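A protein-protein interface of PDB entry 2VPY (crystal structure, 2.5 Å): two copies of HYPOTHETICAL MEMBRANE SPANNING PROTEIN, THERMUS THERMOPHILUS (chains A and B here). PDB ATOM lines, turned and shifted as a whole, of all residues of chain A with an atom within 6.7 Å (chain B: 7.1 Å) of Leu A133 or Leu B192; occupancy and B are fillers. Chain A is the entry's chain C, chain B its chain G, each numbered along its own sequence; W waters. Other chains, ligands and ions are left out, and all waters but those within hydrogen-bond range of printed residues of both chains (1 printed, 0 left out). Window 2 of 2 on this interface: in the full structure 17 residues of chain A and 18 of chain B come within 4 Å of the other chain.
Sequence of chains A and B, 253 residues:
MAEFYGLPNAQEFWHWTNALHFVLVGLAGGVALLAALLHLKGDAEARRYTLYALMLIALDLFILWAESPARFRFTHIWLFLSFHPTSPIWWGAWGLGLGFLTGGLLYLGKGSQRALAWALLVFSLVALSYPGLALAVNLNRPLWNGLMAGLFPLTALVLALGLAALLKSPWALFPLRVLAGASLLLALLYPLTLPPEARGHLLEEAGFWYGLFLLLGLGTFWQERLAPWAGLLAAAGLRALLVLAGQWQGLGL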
ATOM      1  N   PRO A  88     -15.837  -5.700 -15.530  1.00  0.00           N
ATOM      2  CA  PRO A  88     -14.666  -6.430 -15.052  1.00  0.00           C
ATOM      3  C   PRO A  88     -14.681  -7.943 -15.081  1.00  0.00           C
ATOM      4  O   PRO A  88     -13.669  -8.564 -15.407  1.00  0.00           O
ATOM      5  CB  PRO A  88     -14.466  -5.877 -13.637  1.00  0.00           C
ATOM      6  CG  PRO A  88     -15.041  -4.489 -13.674  1.00  0.00           C
ATOM      7  CD  PRO A  88     -15.735  -4.309 -15.054  1.00  0.00           C
ATOM      8  N   SER A 129      -5.599  -7.476 -12.728  1.00  0.00           N
ATOM      9  CA  SER A 129      -6.297  -6.201 -12.733  1.00  0.00           C
ATOM     10  C   SER A 129      -7.806  -6.224 -12.544  1.00  0.00           C
ATOM     11  O   SER A 129      -8.372  -5.281 -12.001  1.00  0.00           O
ATOM     12  CB  SER A 129      -6.017  -5.482 -14.069  1.00  0.00           C
ATOM     13  OG  SER A 129      -4.704  -5.004 -14.179  1.00  0.00           O
ATOM     14  N   TYR A 130      -8.461  -7.287 -12.974  1.00  0.00           N
ATOM     15  CA  TYR A 130      -9.908  -7.312 -12.903  1.00  0.00           C
ATOM     16  C   TYR A 130     -10.586  -7.394 -11.515  1.00  0.00           C
ATOM     17  O   TYR A 130     -11.655  -6.827 -11.324  1.00  0.00           O
ATOM     18  CB  TYR A 130     -10.465  -8.360 -13.891  1.00  0.00           C
ATOM     19  CG  TYR A 130     -10.959  -9.646 -13.273  1.00  0.00           C
ATOM     20  CD1 TYR A 130     -12.260  -9.751 -12.769  1.00  0.00           C
ATOM     21  CD2 TYR A 130     -10.123 -10.759 -13.177  1.00  0.00           C
ATOM     22  CE1 TYR A 130     -12.722 -10.938 -12.182  1.00  0.00           C
ATOM     23  CE2 TYR A 130     -10.576 -11.959 -12.586  1.00  0.00           C
ATOM     24  CZ  TYR A 130     -11.872 -12.041 -12.092  1.00  0.00           C
ATOM     25  OH  TYR A 130     -12.308 -13.204 -11.504  1.00  0.00           O
ATOM     26  N   PRO A 131      -9.964  -8.094 -10.535  1.00  0.00           N
ATOM     27  CA  PRO A 131     -10.590  -8.159  -9.202  1.00  0.00           C
ATOM     28  C   PRO A 131     -10.793  -6.808  -8.497  1.00  0.00           C
ATOM     29  O   PRO A 131     -11.890  -6.531  -8.014  1.00  0.00           O
ATOM     30  CB  PRO A 131      -9.682  -9.081  -8.403  1.00  0.00           C
ATOM     31  CG  PRO A 131      -9.049  -9.962  -9.436  1.00  0.00           C
ATOM     32  CD  PRO A 131      -8.877  -9.085 -10.667  1.00  0.00           C
ATOM     33  N   GLY A 132      -9.746  -5.988  -8.426  1.00  0.00           N
ATOM     34  CA  GLY A 132      -9.856  -4.685  -7.789  1.00  0.00           C
ATOM     35  C   GLY A 132     -10.873  -3.809  -8.492  1.00  0.00           C
ATOM     36  O   GLY A 132     -11.542  -2.973  -7.868  1.00  0.00           O
ATOM     37  N   LEU A 133     -11.001  -3.987  -9.802  1.00  0.00           N
ATOM     38  CA  LEU A 133     -11.979  -3.219 -10.569  1.00  0.00           C
ATOM     39  C   LEU A 133     -13.390  -3.820 -10.428  1.00  0.00           C
ATOM     40  O   LEU A 133     -14.371  -3.103 -10.590  1.00  0.00           O
ATOM     41  CB  LEU A 133     -11.578  -3.094 -12.064  1.00  0.00           C
ATOM     42  CG  LEU A 133     -10.343  -2.248 -12.432  1.00  0.00           C
ATOM     43  CD1 LEU A 133     -10.171  -2.219 -13.954  1.00  0.00           C
ATOM     44  CD2 LEU A 133     -10.480  -0.821 -11.891  1.00  0.00           C
ATOM     45  N   ALA A 134     -13.501  -5.120 -10.126  1.00  0.00           N
ATOM     46  CA  ALA A 134     -14.822  -5.739  -9.933  1.00  0.00           C
ATOM     47  C   ALA A 134     -15.427  -5.112  -8.661  1.00  0.00           C
ATOM     48  O   ALA A 134     -16.654  -4.992  -8.533  1.00  0.00           O
ATOM     49  CB  ALA A 134     -14.719  -7.283  -9.783  1.00  0.00           C
ATOM     50  N   LEU A 135     -14.558  -4.704  -7.734  1.00  0.00           N
ATOM     51  CA  LEU A 135     -14.966  -4.021  -6.507  1.00  0.00           C
ATOM     52  C   LEU A 135     -15.199  -2.518  -6.766  1.00  0.00           C
ATOM     53  O   LEU A 135     -16.324  -2.011  -6.611  1.00  0.00           O
ATOM     54  CB  LEU A 135     -13.887  -4.139  -5.403  1.00  0.00           C
ATOM     55  CG  LEU A 135     -13.440  -5.541  -4.986  1.00  0.00           C
ATOM     56  CD1 LEU A 135     -12.692  -5.499  -3.640  1.00  0.00           C
ATOM     57  CD2 LEU A 135     -14.663  -6.471  -4.888  1.00  0.00           C
ATOM     58  N   ALA A 136     -14.114  -1.857  -7.163  1.00  0.00           N
ATOM     59  CA  ALA A 136     -14.009  -0.411  -7.426  1.00  0.00           C
ATOM     60  C   ALA A 136     -14.973   0.315  -8.365  1.00  0.00           C
ATOM     61  O   ALA A 136     -15.117   1.532  -8.283  1.00  0.00           O
ATOM     62  CB  ALA A 136     -12.548  -0.070  -7.812  1.00  0.00           C
ATOM     63  N   VAL A 137     -15.612  -0.413  -9.270  1.00  0.00           N
ATOM     64  CA  VAL A 137     -16.579   0.191 -10.201  1.00  0.00           C
ATOM     65  C   VAL A 137     -17.922   0.482  -9.527  1.00  0.00           C
ATOM     66  O   VAL A 137     -18.770   1.211 -10.069  1.00  0.00           O
ATOM     67  CB  VAL A 137     -16.871  -0.719 -11.448  1.00  0.00           C
ATOM     68  CG1 VAL A 137     -15.675  -0.727 -12.403  1.00  0.00           C
ATOM     69  CG2 VAL A 137     -17.211  -2.132 -10.987  1.00  0.00           C
ATOM     70  N   ASN A 138     -18.116  -0.120  -8.348  1.00  0.00           N
ATOM     71  CA  ASN A 138     -19.344   0.058  -7.551  1.00  0.00           C
ATOM     72  C   ASN A 138     -19.172   1.245  -6.655  1.00  0.00           C
ATOM     73  O   ASN A 138     -18.884   1.117  -5.455  1.00  0.00           O
ATOM     74  CB  ASN A 138     -19.579  -1.186  -6.721  1.00  0.00           C
ATOM     75  CG  ASN A 138     -19.541  -2.428  -7.542  1.00  0.00           C
ATOM     76  OD1 ASN A 138     -18.781  -3.355  -7.265  1.00  0.00           O
ATOM     77  ND2 ASN A 138     -20.330  -2.438  -8.604  1.00  0.00           N
ATOM     78  N   GLY A 146     -11.276   3.752  -5.115  1.00  0.00           N
ATOM     79  CA  GLY A 146     -10.178   3.623  -6.058  1.00  0.00           C
ATOM     80  C   GLY A 146      -8.962   2.791  -5.643  1.00  0.00           C
ATOM     81  O   GLY A 146      -8.413   2.083  -6.480  1.00  0.00           O
ATOM     82  N   MET A 148      -8.751   0.082  -4.264  1.00  0.00           N
ATOM     83  CA  MET A 148      -9.012  -1.337  -4.483  1.00  0.00           C
ATOM     84  C   MET A 148      -8.347  -1.745  -5.797  1.00  0.00           C
ATOM     85  O   MET A 148      -7.961  -2.911  -5.988  1.00  0.00           O
ATOM     86  CB  MET A 148     -10.514  -1.630  -4.562  1.00  0.00           C
ATOM     87  CG  MET A 148     -11.290  -1.321  -3.288  1.00  0.00           C
ATOM     88  SD  MET A 148     -10.736  -2.295  -1.875  1.00  0.00           S
ATOM     89  CE  MET A 148     -10.083  -0.978  -0.803  1.00  0.00           C
ATOM     90  N   ALA A 149      -8.242  -0.788  -6.717  1.00  0.00           N
ATOM     91  CA  ALA A 149      -7.597  -1.047  -7.993  1.00  0.00           C
ATOM     92  C   ALA A 149      -6.059  -1.058  -7.776  1.00  0.00           C
ATOM     93  O   ALA A 149      -5.311  -1.463  -8.662  1.00  0.00           O
ATOM     94  CB  ALA A 149      -7.989   0.015  -9.038  1.00  0.00           C
ATOM     95  N   PHE A 152      -5.569  -4.584  -4.893  1.00  0.00           N
ATOM     96  CA  PHE A 152      -5.692  -5.935  -5.386  1.00  0.00           C
ATOM     97  C   PHE A 152      -4.534  -6.432  -6.280  1.00  0.00           C
ATOM     98  O   PHE A 152      -4.081  -7.565  -6.097  1.00  0.00           O
ATOM     99  CB  PHE A 152      -7.128  -6.207  -5.862  1.00  0.00           C
ATOM    100  CG  PHE A 152      -8.085  -6.542  -4.729  1.00  0.00           C
ATOM    101  CD1 PHE A 152      -8.405  -5.584  -3.768  1.00  0.00           C
ATOM    102  CD2 PHE A 152      -8.591  -7.840  -4.578  1.00  0.00           C
ATOM    103  CE1 PHE A 152      -9.216  -5.899  -2.669  1.00  0.00           C
ATOM    104  CE2 PHE A 152      -9.408  -8.173  -3.476  1.00  0.00           C
ATOM    105  CZ  PHE A 152      -9.719  -7.198  -2.519  1.00  0.00           C
ATOM    106  N   PRO A 153      -4.029  -5.603  -7.222  1.00  0.00           N
ATOM    107  CA  PRO A 153      -2.898  -6.055  -8.047  1.00  0.00           C
ATOM    108  C   PRO A 153      -1.599  -6.319  -7.209  1.00  0.00           C
ATOM    109  O   PRO A 153      -0.908  -7.321  -7.399  1.00  0.00           O
ATOM    110  CB  PRO A 153      -2.702  -4.919  -9.037  1.00  0.00           C
ATOM    111  CG  PRO A 153      -4.093  -4.436  -9.286  1.00  0.00           C
ATOM    112  CD  PRO A 153      -4.791  -4.545  -7.913  1.00  0.00           C
ATOM    113  N   ALA B 187      -1.576   3.255 -12.777  1.00  0.00           N
ATOM    114  CA  ALA B 187      -1.818   4.519 -13.491  1.00  0.00           C
ATOM    115  C   ALA B 187      -2.775   4.348 -14.671  1.00  0.00           C
ATOM    116  O   ALA B 187      -3.517   5.263 -15.041  1.00  0.00           O
ATOM    117  CB  ALA B 187      -0.495   5.145 -13.958  1.00  0.00           C
ATOM    118  N   LEU B 188      -2.760   3.149 -15.227  1.00  0.00           N
ATOM    119  CA  LEU B 188      -3.616   2.749 -16.341  1.00  0.00           C
ATOM    120  C   LEU B 188      -5.058   2.455 -15.861  1.00  0.00           C
ATOM    121  O   LEU B 188      -6.041   2.741 -16.554  1.00  0.00           O
ATOM    122  CB  LEU B 188      -3.024   1.494 -16.979  1.00  0.00           C
ATOM    123  CG  LEU B 188      -3.753   0.834 -18.135  1.00  0.00           C
ATOM    124  CD1 LEU B 188      -3.794   1.755 -19.343  1.00  0.00           C
ATOM    125  CD2 LEU B 188      -3.038  -0.464 -18.470  1.00  0.00           C
ATOM    126  N   LEU B 189      -5.161   1.870 -14.669  1.00  0.00           N
ATOM    127  CA  LEU B 189      -6.440   1.511 -14.059  1.00  0.00           C
ATOM    128  C   LEU B 189      -7.151   2.723 -13.463  1.00  0.00           C
ATOM    129  O   LEU B 189      -8.377   2.766 -13.420  1.00  0.00           O
ATOM    130  CB  LEU B 189      -6.236   0.407 -13.000  1.00  0.00           C
ATOM    131  CG  LEU B 189      -5.611  -0.920 -13.477  1.00  0.00           C
ATOM    132  CD1 LEU B 189      -5.634  -1.949 -12.343  1.00  0.00           C
ATOM    133  CD2 LEU B 189      -6.358  -1.456 -14.691  1.00  0.00           C
ATOM    134  N   TYR B 190      -6.386   3.710 -13.016  1.00  0.00           N
ATOM    135  CA  TYR B 190      -6.948   4.935 -12.450  1.00  0.00           C
ATOM    136  C   TYR B 190      -8.196   5.516 -13.217  1.00  0.00           C
ATOM    137  O   TYR B 190      -9.267   5.669 -12.612  1.00  0.00           O
ATOM    138  CB  TYR B 190      -5.833   5.986 -12.303  1.00  0.00           C
ATOM    139  CG  TYR B 190      -6.355   7.307 -11.845  1.00  0.00           C
ATOM    140  CD1 TYR B 190      -6.943   7.454 -10.588  1.00  0.00           C
ATOM    141  CD2 TYR B 190      -6.321   8.405 -12.697  1.00  0.00           C
ATOM    142  CE1 TYR B 190      -7.488   8.665 -10.194  1.00  0.00           C
ATOM    143  CE2 TYR B 190      -6.859   9.618 -12.318  1.00  0.00           C
ATOM    144  CZ  TYR B 190      -7.440   9.744 -11.072  1.00  0.00           C
ATOM    145  OH  TYR B 190      -7.965  10.960 -10.737  1.00  0.00           O
ATOM    146  N   PRO B 191      -8.083   5.856 -14.530  1.00  0.00           N
ATOM    147  CA  PRO B 191      -9.255   6.392 -15.255  1.00  0.00           C
ATOM    148  C   PRO B 191     -10.558   5.564 -15.153  1.00  0.00           C
ATOM    149  O   PRO B 191     -11.674   6.097 -15.196  1.00  0.00           O
ATOM    150  CB  PRO B 191      -8.784   6.432 -16.708  1.00  0.00           C
ATOM    151  CG  PRO B 191      -7.339   6.765 -16.597  1.00  0.00           C
ATOM    152  CD  PRO B 191      -6.856   6.022 -15.337  1.00  0.00           C
ATOM    153  N   LEU B 192     -10.387   4.255 -15.042  1.00  0.00           N
ATOM    154  CA  LEU B 192     -11.480   3.270 -14.993  1.00  0.00           C
ATOM    155  C   LEU B 192     -12.187   3.137 -13.650  1.00  0.00           C
ATOM    156  O   LEU B 192     -13.163   2.405 -13.475  1.00  0.00           O
ATOM    157  CB  LEU B 192     -10.923   1.904 -15.369  1.00  0.00           C
ATOM    158  CG  LEU B 192     -10.294   1.699 -16.735  1.00  0.00           C
ATOM    159  CD1 LEU B 192      -9.966   0.216 -16.852  1.00  0.00           C
ATOM    160  CD2 LEU B 192     -11.245   2.135 -17.856  1.00  0.00           C
ATOM    161  N   THR B 193     -11.659   3.907 -12.734  1.00  0.00           N
ATOM    162  CA  THR B 193     -11.996   3.992 -11.341  1.00  0.00           C
ATOM    163  C   THR B 193     -12.844   5.222 -11.006  1.00  0.00           C
ATOM    164  O   THR B 193     -13.408   5.333  -9.908  1.00  0.00           O
ATOM    165  CB  THR B 193     -10.625   4.071 -10.647  1.00  0.00           C
ATOM    166  OG1 THR B 193     -10.279   2.815 -10.073  1.00  0.00           O
ATOM    167  CG2 THR B 193     -10.570   5.215  -9.683  1.00  0.00           C
ATOM    168  N   LEU B 194     -12.911   6.149 -11.948  1.00  0.00           N
ATOM    169  CA  LEU B 194     -13.612   7.411 -11.747  1.00  0.00           C
ATOM    170  C   LEU B 194     -15.049   7.430 -12.214  1.00  0.00           C
ATOM    171  O   LEU B 194     -15.452   6.568 -12.992  1.00  0.00           O
ATOM    172  CB  LEU B 194     -12.875   8.517 -12.497  1.00  0.00           C
ATOM    173  CG  LEU B 194     -11.431   8.779 -12.066  1.00  0.00           C
ATOM    174  CD1 LEU B 194     -10.771   9.683 -13.103  1.00  0.00           C
ATOM    175  CD2 LEU B 194     -11.393   9.394 -10.652  1.00  0.00           C
ATOM    176  N   PRO B 195     -15.866   8.368 -11.695  1.00  0.00           N
ATOM    177  CA  PRO B 195     -17.192   8.246 -12.291  1.00  0.00           C
ATOM    178  C   PRO B 195     -17.067   8.798 -13.735  1.00  0.00           C
ATOM    179  O   PRO B 195     -16.118   9.533 -14.053  1.00  0.00           O
ATOM    180  CB  PRO B 195     -18.101   9.066 -11.365  1.00  0.00           C
ATOM    181  CG  PRO B 195     -17.180   9.878 -10.493  1.00  0.00           C
ATOM    182  CD  PRO B 195     -15.859   9.163 -10.452  1.00  0.00           C
ATOM    183  N   ARG B 199     -13.982  11.159 -15.277  1.00  0.00           N
ATOM    184  CA  ARG B 199     -13.084  10.583 -16.260  1.00  0.00           C
ATOM    185  C   ARG B 199     -13.080  11.411 -17.539  1.00  0.00           C
ATOM    186  O   ARG B 199     -12.025  11.647 -18.136  1.00  0.00           O
ATOM    187  CB  ARG B 199     -13.472   9.160 -16.641  1.00  0.00           C
ATOM    188  CG  ARG B 199     -12.566   8.599 -17.758  1.00  0.00           C
ATOM    189  CD  ARG B 199     -13.139   7.333 -18.314  1.00  0.00           C
ATOM    190  NE  ARG B 199     -13.536   6.501 -17.194  1.00  0.00           N
ATOM    191  CZ  ARG B 199     -14.711   5.902 -17.067  1.00  0.00           C
ATOM    192  NH1 ARG B 199     -15.624   6.027 -18.017  1.00  0.00           N
ATOM    193  NH2 ARG B 199     -14.989   5.222 -15.958  1.00  0.00           N
ATOM    194  N   LEU B 202     -11.053  14.333 -17.075  1.00  0.00           N
ATOM    195  CA  LEU B 202      -9.644  13.998 -17.103  1.00  0.00           C
ATOM    196  C   LEU B 202      -9.141  13.799 -18.535  1.00  0.00           C
ATOM    197  O   LEU B 202      -8.109  14.361 -18.902  1.00  0.00           O
ATOM    198  CB  LEU B 202      -9.346  12.761 -16.248  1.00  0.00           C
ATOM    199  CG  LEU B 202      -7.939  12.167 -16.358  1.00  0.00           C
ATOM    200  CD1 LEU B 202      -6.914  13.013 -15.575  1.00  0.00           C
ATOM    201  CD2 LEU B 202      -7.987  10.717 -15.858  1.00  0.00           C
HETATM  202  O   HOH W   1     -13.725   3.616  -7.504  1.00  0.00           O
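Among the printed residues, merely in contact across the chains: Ser A129 with Leu B189, Leu A133 with Leu B189, Leu A133 with Leu B192, Gly A146 with Thr B193, Ala A149 with Leu B189 and Ala A149 with Thr B193.
No residue of chain B comes within 4 Å of Gly A132.
Leu A135 touches none of the printed residues of chain B.
Of the printed residues of chain B, Gly A146 touches Thr B193 (3.98 Å).
Printed residues of chain A within 4 Å of Thr B193: Gly A146 and Ala A149.
The nearest printed residue of chain B that does not touch Gly A146 is Tyr B190 (6.8 Å).
Printed residues of chain B that touch a printed residue of chain A: Leu B189, Leu B192 and Thr B193.
Hydrophobic or aromatic side chains of chain B within 4 Å of the printed part of chain A: Leu B189 and Leu B192.
Of the 16 printed residues of chain A, 4 touch a printed residue of chain B.
Among the printed residues, 6 pairs touch across the chains.
No position is printed for both chains.
Of the 6 pairs that touch across the chains among the printed residues, none has its exchanged pair printed and touching as well.
Water W1 lies within hydrogen-bond range of the backbone carbonyl oxygen of Ala A136 (2.6 Å), the backbone carbonyl oxygen of Thr B193 (3.0 Å) and the backbone NH of Gly A146 (3.4 Å).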
